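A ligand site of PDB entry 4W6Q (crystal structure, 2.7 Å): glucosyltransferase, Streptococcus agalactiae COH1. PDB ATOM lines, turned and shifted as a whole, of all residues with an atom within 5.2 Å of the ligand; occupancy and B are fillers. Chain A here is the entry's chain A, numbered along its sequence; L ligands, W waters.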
ATOM      1  N   THR A  18      16.762 -20.942 -24.487  1.00  0.00           N
ATOM      2  CA  THR A  18      15.978 -21.572 -25.537  1.00  0.00           C
ATOM      3  C   THR A  18      16.471 -21.158 -26.911  1.00  0.00           C
ATOM      4  O   THR A  18      16.531 -21.961 -27.827  1.00  0.00           O
ATOM      5  CB  THR A  18      14.483 -21.249 -25.389  1.00  0.00           C
ATOM      6  OG1 THR A  18      13.996 -21.791 -24.148  1.00  0.00           O
ATOM      7  CG2 THR A  18      13.677 -21.808 -26.549  1.00  0.00           C
ATOM      8  N   HIS A 158      11.517 -31.005 -33.128  1.00  0.00           N
ATOM      9  CA  HIS A 158      11.994 -31.456 -31.842  1.00  0.00           C
ATOM     10  C   HIS A 158      12.547 -32.879 -32.004  1.00  0.00           C
ATOM     11  O   HIS A 158      11.901 -33.849 -31.614  1.00  0.00           O
ATOM     12  CB  HIS A 158      10.881 -31.406 -30.805  1.00  0.00           C
ATOM     13  CG  HIS A 158      11.365 -31.352 -29.390  1.00  0.00           C
ATOM     14  ND1 HIS A 158      11.069 -30.303 -28.547  1.00  0.00           N
ATOM     15  CD2 HIS A 158      12.135 -32.206 -28.686  1.00  0.00           C
ATOM     16  CE1 HIS A 158      11.637 -30.528 -27.367  1.00  0.00           C
ATOM     17  NE2 HIS A 158      12.291 -31.674 -27.430  1.00  0.00           N
ATOM     18  N   PRO A 176       5.521 -26.148 -19.694  1.00  0.00           N
ATOM     19  CA  PRO A 176       6.934 -25.993 -19.383  1.00  0.00           C
ATOM     20  C   PRO A 176       7.397 -24.593 -19.750  1.00  0.00           C
ATOM     21  O   PRO A 176       7.953 -24.383 -20.816  1.00  0.00           O
ATOM     22  CB  PRO A 176       7.603 -27.055 -20.244  1.00  0.00           C
ATOM     23  CG  PRO A 176       6.705 -27.168 -21.445  1.00  0.00           C
ATOM     24  CD  PRO A 176       5.315 -26.775 -21.006  1.00  0.00           C
ATOM     25  N   GLY A 177       7.125 -23.637 -18.865  1.00  0.00           N
ATOM     26  CA  GLY A 177       7.478 -22.264 -19.143  1.00  0.00           C
ATOM     27  C   GLY A 177       7.708 -21.439 -17.900  1.00  0.00           C
ATOM     28  O   GLY A 177       6.852 -21.371 -17.015  1.00  0.00           O
ATOM     29  N   ARG A 181       7.559 -14.808 -17.136  1.00  0.00           N
ATOM     30  CA  ARG A 181       7.486 -14.383 -18.507  1.00  0.00           C
ATOM     31  C   ARG A 181       6.014 -14.425 -18.865  1.00  0.00           C
ATOM     32  O   ARG A 181       5.526 -13.634 -19.657  1.00  0.00           O
ATOM     33  CB  ARG A 181       8.340 -15.299 -19.399  1.00  0.00           C
ATOM     34  CG  ARG A 181       8.525 -14.863 -20.839  1.00  0.00           C
ATOM     35  CD  ARG A 181       9.448 -15.840 -21.542  1.00  0.00           C
ATOM     36  NE  ARG A 181       9.100 -16.003 -22.949  1.00  0.00           N
ATOM     37  CZ  ARG A 181       9.745 -16.813 -23.776  1.00  0.00           C
ATOM     38  NH1 ARG A 181      10.768 -17.534 -23.318  1.00  0.00           N
ATOM     39  NH2 ARG A 181       9.372 -16.907 -25.048  1.00  0.00           N
ATOM     40  N   PHE A 182       5.302 -15.333 -18.205  1.00  0.00           N
ATOM     41  CA  PHE A 182       3.883 -15.547 -18.466  1.00  0.00           C
ATOM     42  C   PHE A 182       3.064 -15.251 -17.224  1.00  0.00           C
ATOM     43  O   PHE A 182       3.024 -16.066 -16.308  1.00  0.00           O
ATOM     44  CB  PHE A 182       3.626 -16.988 -18.919  1.00  0.00           C
ATOM     45  CG  PHE A 182       4.532 -17.463 -20.022  1.00  0.00           C
ATOM     46  CD1 PHE A 182       4.222 -17.235 -21.347  1.00  0.00           C
ATOM     47  CD2 PHE A 182       5.677 -18.186 -19.721  1.00  0.00           C
ATOM     48  CE1 PHE A 182       5.044 -17.705 -22.358  1.00  0.00           C
ATOM     49  CE2 PHE A 182       6.507 -18.660 -20.730  1.00  0.00           C
ATOM     50  CZ  PHE A 182       6.193 -18.418 -22.053  1.00  0.00           C
ATOM     51  N   TYR A 197       6.588 -26.511 -15.164  1.00  0.00           N
ATOM     52  CA  TYR A 197       7.940 -27.035 -15.109  1.00  0.00           C
ATOM     53  C   TYR A 197       8.881 -25.870 -15.147  1.00  0.00           C
ATOM     54  O   TYR A 197       9.057 -25.235 -16.186  1.00  0.00           O
ATOM     55  CB  TYR A 197       8.198 -28.008 -16.257  1.00  0.00           C
ATOM     56  CG  TYR A 197       7.123 -29.076 -16.390  1.00  0.00           C
ATOM     57  CD1 TYR A 197       5.915 -28.799 -17.017  1.00  0.00           C
ATOM     58  CD2 TYR A 197       7.325 -30.346 -15.870  1.00  0.00           C
ATOM     59  CE1 TYR A 197       4.935 -29.760 -17.120  1.00  0.00           C
ATOM     60  CE2 TYR A 197       6.341 -31.323 -15.988  1.00  0.00           C
ATOM     61  CZ  TYR A 197       5.156 -31.022 -16.614  1.00  0.00           C
ATOM     62  OH  TYR A 197       4.179 -31.981 -16.726  1.00  0.00           O
ATOM     63  N   THR A 198       9.479 -25.566 -14.007  1.00  0.00           N
ATOM     64  CA  THR A 198      10.321 -24.396 -13.934  1.00  0.00           C
ATOM     65  C   THR A 198      11.401 -24.497 -12.883  1.00  0.00           C
ATOM     66  O   THR A 198      11.208 -25.059 -11.802  1.00  0.00           O
ATOM     67  CB  THR A 198       9.477 -23.148 -13.684  1.00  0.00           C
ATOM     68  OG1 THR A 198      10.300 -21.982 -13.874  1.00  0.00           O
ATOM     69  CG2 THR A 198       8.900 -23.164 -12.285  1.00  0.00           C
ATOM     70  N   PRO A 212      10.019 -29.007 -10.599  1.00  0.00           N
ATOM     71  CA  PRO A 212      11.373 -28.564 -10.918  1.00  0.00           C
ATOM     72  C   PRO A 212      11.813 -29.008 -12.305  1.00  0.00           C
ATOM     73  O   PRO A 212      11.552 -30.136 -12.726  1.00  0.00           O
ATOM     74  CB  PRO A 212      12.224 -29.222  -9.818  1.00  0.00           C
ATOM     75  CG  PRO A 212      11.465 -30.437  -9.438  1.00  0.00           C
ATOM     76  CD  PRO A 212      10.001 -30.074  -9.581  1.00  0.00           C
ATOM     77  N   TYR A 213      12.474 -28.078 -12.998  1.00  0.00           N
ATOM     78  CA  TYR A 213      13.031 -28.211 -14.338  1.00  0.00           C
ATOM     79  C   TYR A 213      13.573 -29.585 -14.727  1.00  0.00           C
ATOM     80  O   TYR A 213      14.689 -29.928 -14.387  1.00  0.00           O
ATOM     81  CB  TYR A 213      14.142 -27.183 -14.501  1.00  0.00           C
ATOM     82  CG  TYR A 213      14.517 -26.906 -15.928  1.00  0.00           C
ATOM     83  CD1 TYR A 213      15.519 -27.635 -16.555  1.00  0.00           C
ATOM     84  CD2 TYR A 213      13.873 -25.929 -16.654  1.00  0.00           C
ATOM     85  CE1 TYR A 213      15.868 -27.392 -17.880  1.00  0.00           C
ATOM     86  CE2 TYR A 213      14.214 -25.675 -17.968  1.00  0.00           C
ATOM     87  CZ  TYR A 213      15.206 -26.416 -18.579  1.00  0.00           C
ATOM     88  OH  TYR A 213      15.556 -26.167 -19.892  1.00  0.00           O
ATOM     89  N   GLN A 214      12.789 -30.350 -15.486  1.00  0.00           N
ATOM     90  CA  GLN A 214      13.218 -31.676 -15.932  1.00  0.00           C
ATOM     91  C   GLN A 214      14.125 -31.534 -17.162  1.00  0.00           C
ATOM     92  O   GLN A 214      13.996 -30.568 -17.926  1.00  0.00           O
ATOM     93  CB  GLN A 214      12.008 -32.578 -16.273  1.00  0.00           C
ATOM     94  CG  GLN A 214      10.727 -32.396 -15.429  1.00  0.00           C
ATOM     95  CD  GLN A 214      10.805 -33.019 -14.023  1.00  0.00           C
ATOM     96  OE1 GLN A 214      11.817 -32.905 -13.341  1.00  0.00           O
ATOM     97  NE2 GLN A 214       9.719 -33.672 -13.582  1.00  0.00           N
ATOM     98  N   SER A 215      15.058 -32.474 -17.353  1.00  0.00           N
ATOM     99  CA  SER A 215      15.798 -32.533 -18.612  1.00  0.00           C
ATOM    100  C   SER A 215      14.773 -32.825 -19.697  1.00  0.00           C
ATOM    101  O   SER A 215      13.786 -33.513 -19.446  1.00  0.00           O
ATOM    102  CB  SER A 215      16.832 -33.633 -18.571  1.00  0.00           C
ATOM    103  OG  SER A 215      17.199 -33.880 -17.234  1.00  0.00           O
ATOM    104  N   ASP A 216      15.000 -32.307 -20.894  1.00  0.00           N
ATOM    105  CA  ASP A 216      13.944 -32.360 -21.896  1.00  0.00           C
ATOM    106  C   ASP A 216      13.440 -33.767 -22.161  1.00  0.00           C
ATOM    107  O   ASP A 216      12.243 -34.025 -22.150  1.00  0.00           O
ATOM    108  CB  ASP A 216      14.405 -31.745 -23.215  1.00  0.00           C
ATOM    109  CG  ASP A 216      13.265 -31.569 -24.173  1.00  0.00           C
ATOM    110  OD1 ASP A 216      12.604 -30.508 -24.120  1.00  0.00           O
ATOM    111  OD2 ASP A 216      13.004 -32.502 -24.958  1.00  0.00           O
ATOM    112  N   LEU A 219      11.093 -34.766 -19.734  1.00  0.00           N
ATOM    113  CA  LEU A 219       9.899 -33.947 -19.817  1.00  0.00           C
ATOM    114  C   LEU A 219       8.961 -34.487 -20.895  1.00  0.00           C
ATOM    115  O   LEU A 219       7.741 -34.528 -20.719  1.00  0.00           O
ATOM    116  CB  LEU A 219      10.258 -32.485 -20.128  1.00  0.00           C
ATOM    117  CG  LEU A 219       9.086 -31.600 -20.564  1.00  0.00           C
ATOM    118  CD1 LEU A 219       8.095 -31.455 -19.427  1.00  0.00           C
ATOM    119  CD2 LEU A 219       9.564 -30.237 -21.040  1.00  0.00           C
ATOM    120  N   MET A 233       1.077 -17.199 -24.283  1.00  0.00           N
ATOM    121  CA  MET A 233       2.135 -16.231 -24.570  1.00  0.00           C
ATOM    122  C   MET A 233       1.433 -14.913 -24.678  1.00  0.00           C
ATOM    123  O   MET A 233       0.267 -14.879 -25.055  1.00  0.00           O
ATOM    124  CB  MET A 233       2.883 -16.584 -25.888  1.00  0.00           C
ATOM    125  CG  MET A 233       4.114 -15.739 -26.213  1.00  0.00           C
ATOM    126  SD  MET A 233       5.371 -16.523 -27.243  1.00  0.00           S
ATOM    127  CE  MET A 233       6.032 -17.738 -26.114  1.00  0.00           C
ATOM    128  N   TYR A 244       6.446 -15.560 -34.441  1.00  0.00           N
ATOM    129  CA  TYR A 244       7.399 -16.668 -34.469  1.00  0.00           C
ATOM    130  C   TYR A 244       6.782 -18.009 -34.041  1.00  0.00           C
ATOM    131  O   TYR A 244       5.623 -18.111 -33.635  1.00  0.00           O
ATOM    132  CB  TYR A 244       8.664 -16.355 -33.627  1.00  0.00           C
ATOM    133  CG  TYR A 244       8.540 -16.202 -32.109  1.00  0.00           C
ATOM    134  CD1 TYR A 244       8.302 -17.300 -31.281  1.00  0.00           C
ATOM    135  CD2 TYR A 244       8.760 -14.971 -31.498  1.00  0.00           C
ATOM    136  CE1 TYR A 244       8.221 -17.156 -29.891  1.00  0.00           C
ATOM    137  CE2 TYR A 244       8.685 -14.817 -30.114  1.00  0.00           C
ATOM    138  CZ  TYR A 244       8.406 -15.919 -29.321  1.00  0.00           C
ATOM    139  OH  TYR A 244       8.330 -15.772 -27.949  1.00  0.00           O
ATOM    140  N   CYS A 245       7.586 -19.053 -34.197  1.00  0.00           N
ATOM    141  CA  CYS A 245       7.162 -20.396 -33.881  1.00  0.00           C
ATOM    142  C   CYS A 245       7.538 -20.718 -32.439  1.00  0.00           C
ATOM    143  O   CYS A 245       8.671 -20.449 -32.030  1.00  0.00           O
ATOM    144  CB  CYS A 245       7.800 -21.390 -34.865  1.00  0.00           C
ATOM    145  SG  CYS A 245       7.401 -21.093 -36.607  1.00  0.00           S
ATOM    146  N   PRO A 246       6.574 -21.247 -31.648  1.00  0.00           N
ATOM    147  CA  PRO A 246       6.885 -21.653 -30.275  1.00  0.00           C
ATOM    148  C   PRO A 246       7.665 -22.949 -30.267  1.00  0.00           C
ATOM    149  O   PRO A 246       7.428 -23.842 -31.068  1.00  0.00           O
ATOM    150  CB  PRO A 246       5.506 -21.844 -29.624  1.00  0.00           C
ATOM    151  CG  PRO A 246       4.610 -22.139 -30.734  1.00  0.00           C
ATOM    152  CD  PRO A 246       5.144 -21.414 -31.966  1.00  0.00           C
ATOM    153  N   TYR A 247       8.617 -23.021 -29.366  1.00  0.00           N
ATOM    154  CA  TYR A 247       9.414 -24.211 -29.224  1.00  0.00           C
ATOM    155  C   TYR A 247       8.709 -25.243 -28.342  1.00  0.00           C
ATOM    156  O   TYR A 247       9.010 -26.434 -28.415  1.00  0.00           O
ATOM    157  CB  TYR A 247      10.778 -23.835 -28.658  1.00  0.00           C
ATOM    158  CG  TYR A 247      11.681 -25.012 -28.557  1.00  0.00           C
ATOM    159  CD1 TYR A 247      12.226 -25.578 -29.692  1.00  0.00           C
ATOM    160  CD2 TYR A 247      11.962 -25.597 -27.326  1.00  0.00           C
ATOM    161  CE1 TYR A 247      13.043 -26.685 -29.613  1.00  0.00           C
ATOM    162  CE2 TYR A 247      12.783 -26.696 -27.243  1.00  0.00           C
ATOM    163  CZ  TYR A 247      13.324 -27.231 -28.395  1.00  0.00           C
ATOM    164  OH  TYR A 247      14.142 -28.322 -28.333  1.00  0.00           O
ATOM    165  N   LYS A 248       7.779 -24.827 -27.503  1.00  0.00           N
ATOM    166  CA  LYS A 248       7.190 -25.810 -26.618  1.00  0.00           C
ATOM    167  C   LYS A 248       6.080 -26.547 -27.332  1.00  0.00           C
ATOM    168  O   LYS A 248       5.878 -27.733 -27.097  1.00  0.00           O
ATOM    169  CB  LYS A 248       6.712 -25.183 -25.311  1.00  0.00           C
ATOM    170  CG  LYS A 248       5.632 -24.153 -25.423  1.00  0.00           C
ATOM    171  CD  LYS A 248       5.241 -23.700 -24.029  1.00  0.00           C
ATOM    172  CE  LYS A 248       6.195 -22.669 -23.494  1.00  0.00           C
ATOM    173  NZ  LYS A 248       5.832 -21.290 -23.955  1.00  0.00           N
ATOM    174  N   LEU A 249       5.390 -25.834 -28.233  1.00  0.00           N
ATOM    175  CA  LEU A 249       4.387 -26.458 -29.082  1.00  0.00           C
ATOM    176  C   LEU A 249       4.931 -27.719 -29.767  1.00  0.00           C
ATOM    177  O   LEU A 249       4.248 -28.763 -29.851  1.00  0.00           O
ATOM    178  CB  LEU A 249       3.891 -25.470 -30.134  1.00  0.00           C
ATOM    179  CG  LEU A 249       3.186 -26.062 -31.366  1.00  0.00           C
ATOM    180  CD1 LEU A 249       1.848 -26.694 -30.986  1.00  0.00           C
ATOM    181  CD2 LEU A 249       3.007 -25.029 -32.461  1.00  0.00           C
ATOM    182  N   ALA A 251       7.610 -29.203 -28.692  1.00  0.00           N
ATOM    183  CA  ALA A 251       8.024 -30.045 -27.592  1.00  0.00           C
ATOM    184  C   ALA A 251       6.830 -30.886 -27.095  1.00  0.00           C
ATOM    185  O   ALA A 251       6.999 -32.037 -26.677  1.00  0.00           O
ATOM    186  CB  ALA A 251       8.618 -29.187 -26.487  1.00  0.00           C
HETATM  187  N1  LIG L   1      12.194 -27.463 -21.083  1.00  0.00           N
HETATM  188  C1  LIG L   1      13.010 -28.454 -20.574  1.00  0.00           C
HETATM  189  N2  LIG L   1      12.860 -28.849 -19.264  1.00  0.00           N
HETATM  190  C2  LIG L   1      11.878 -28.264 -18.480  1.00  0.00           C
HETATM  191  C3  LIG L   1      11.069 -27.274 -19.029  1.00  0.00           C
HETATM  192  C4  LIG L   1      11.510 -26.664 -20.206  1.00  0.00           C
HETATM  193  O1  LIG L   1      13.862 -28.956 -21.295  1.00  0.00           O
HETATM  194  O2  LIG L   1      11.728 -28.623 -17.311  1.00  0.00           O
HETATM  195  C5  LIG L   1      12.366 -27.058 -22.480  1.00  0.00           C
HETATM  196  C6  LIG L   1      11.163 -27.513 -23.259  1.00  0.00           C
HETATM  197  O3  LIG L   1      11.559 -28.127 -24.461  1.00  0.00           O
HETATM  198  C7  LIG L   1      10.385 -26.232 -23.493  1.00  0.00           C
HETATM  199  C8  LIG L   1      11.458 -25.168 -23.479  1.00  0.00           C
HETATM  200  O4  LIG L   1      12.414 -25.648 -22.566  1.00  0.00           O
HETATM  201  O5  LIG L   1       9.707 -26.307 -24.726  1.00  0.00           O
HETATM  202  C9  LIG L   1      11.023 -23.805 -22.964  1.00  0.00           C
HETATM  203  O6  LIG L   1      10.156 -23.171 -23.871  1.00  0.00           O
HETATM  204  P1  LIG L   1      10.298 -21.599 -24.182  1.00  0.00           P
HETATM  205  O7  LIG L   1      11.667 -21.211 -23.793  1.00  0.00           O
HETATM  206  O8  LIG L   1       9.288 -20.801 -23.447  1.00  0.00           O
HETATM  207  O9  LIG L   1      10.104 -21.513 -25.778  1.00  0.00           O
HETATM  208  P2  LIG L   1       8.738 -21.060 -26.480  1.00  0.00           P
HETATM  209  O10 LIG L   1       8.144 -19.981 -25.667  1.00  0.00           O
HETATM  210  O11 LIG L   1       9.007 -20.598 -27.868  1.00  0.00           O
HETATM  211  O12 LIG L   1       7.768 -22.171 -26.558  1.00  0.00           O
HETATM  212  O   HOH W   1      14.512 -29.356 -25.816  1.00  0.00           O
HETATM  213  O   HOH W   2      10.174 -21.014 -21.050  1.00  0.00           O
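An oxygen (O7) of the ligand lies within hydrogen-bond range of the side-chain hydroxyl of Thr 18, at 2.4 Å. The backbone NH (N) of Gln 214 is in hydrogen-bond range of an oxygen (O2) of the ligand (2.7 Å). The backbone carbonyl oxygen (O) of Gln 214 is in hydrogen-bond range of a nitrogen (N2) of the ligand (2.5 Å). An oxygen (O3) of the ligand lies within hydrogen-bond range of the side-chain carboxylate of Asp 216, 2.6 Å away. An oxygen (O12) of the ligand sits at hydrogen-bond distance from the backbone NH (N) of Lys 248. O10 of the ligand lies within salt-bridge range of NZ of Lys 248 (3.2 Å). An oxygen (O11) of the ligand lies within hydrogen-bond range of the backbone NH (N) of Tyr 247 (2.9 Å). NH2 of Arg 181 is in salt-bridge range of O10 of the ligand (3.4 Å).
OE1 of Gln 214 sits close to O of Pro 212. A ring nitrogen (NE2) of His 158 lies within hydrogen-bond range of the side-chain carboxylate (OD2) of Asp 216 (2.7 Å). SD of Met 233 sits at hydrogen-bond distance from OH of Tyr 244 (3.1 Å). N of Tyr 213 lies within hydrogen-bond range of O of Thr 198, 3.5 Å away. The side-chain hydroxyl (OH) of Tyr 244 lies within hydrogen-bond range of the guanidinium group (NH2) of Arg 181.
Merely in contact with the ligand: His 158, Pro 176, Tyr 197, Tyr 213, Leu 219, Met 233, Pro 246 and Ala 251. Hydrophobic or aromatic side chains within 4 Å of the ligand: His 158, Pro 176, Tyr 197, Tyr 213, Leu 219, Met 233, Pro 246, Tyr 247 and Ala 251.
Water W1 lies within hydrogen-bond range of the side-chain hydroxyl of Tyr 247 (2.7 Å), the side-chain carboxylate of Asp 216 (2.8 Å) and an oxygen (O3) of the ligand (3.5 Å).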
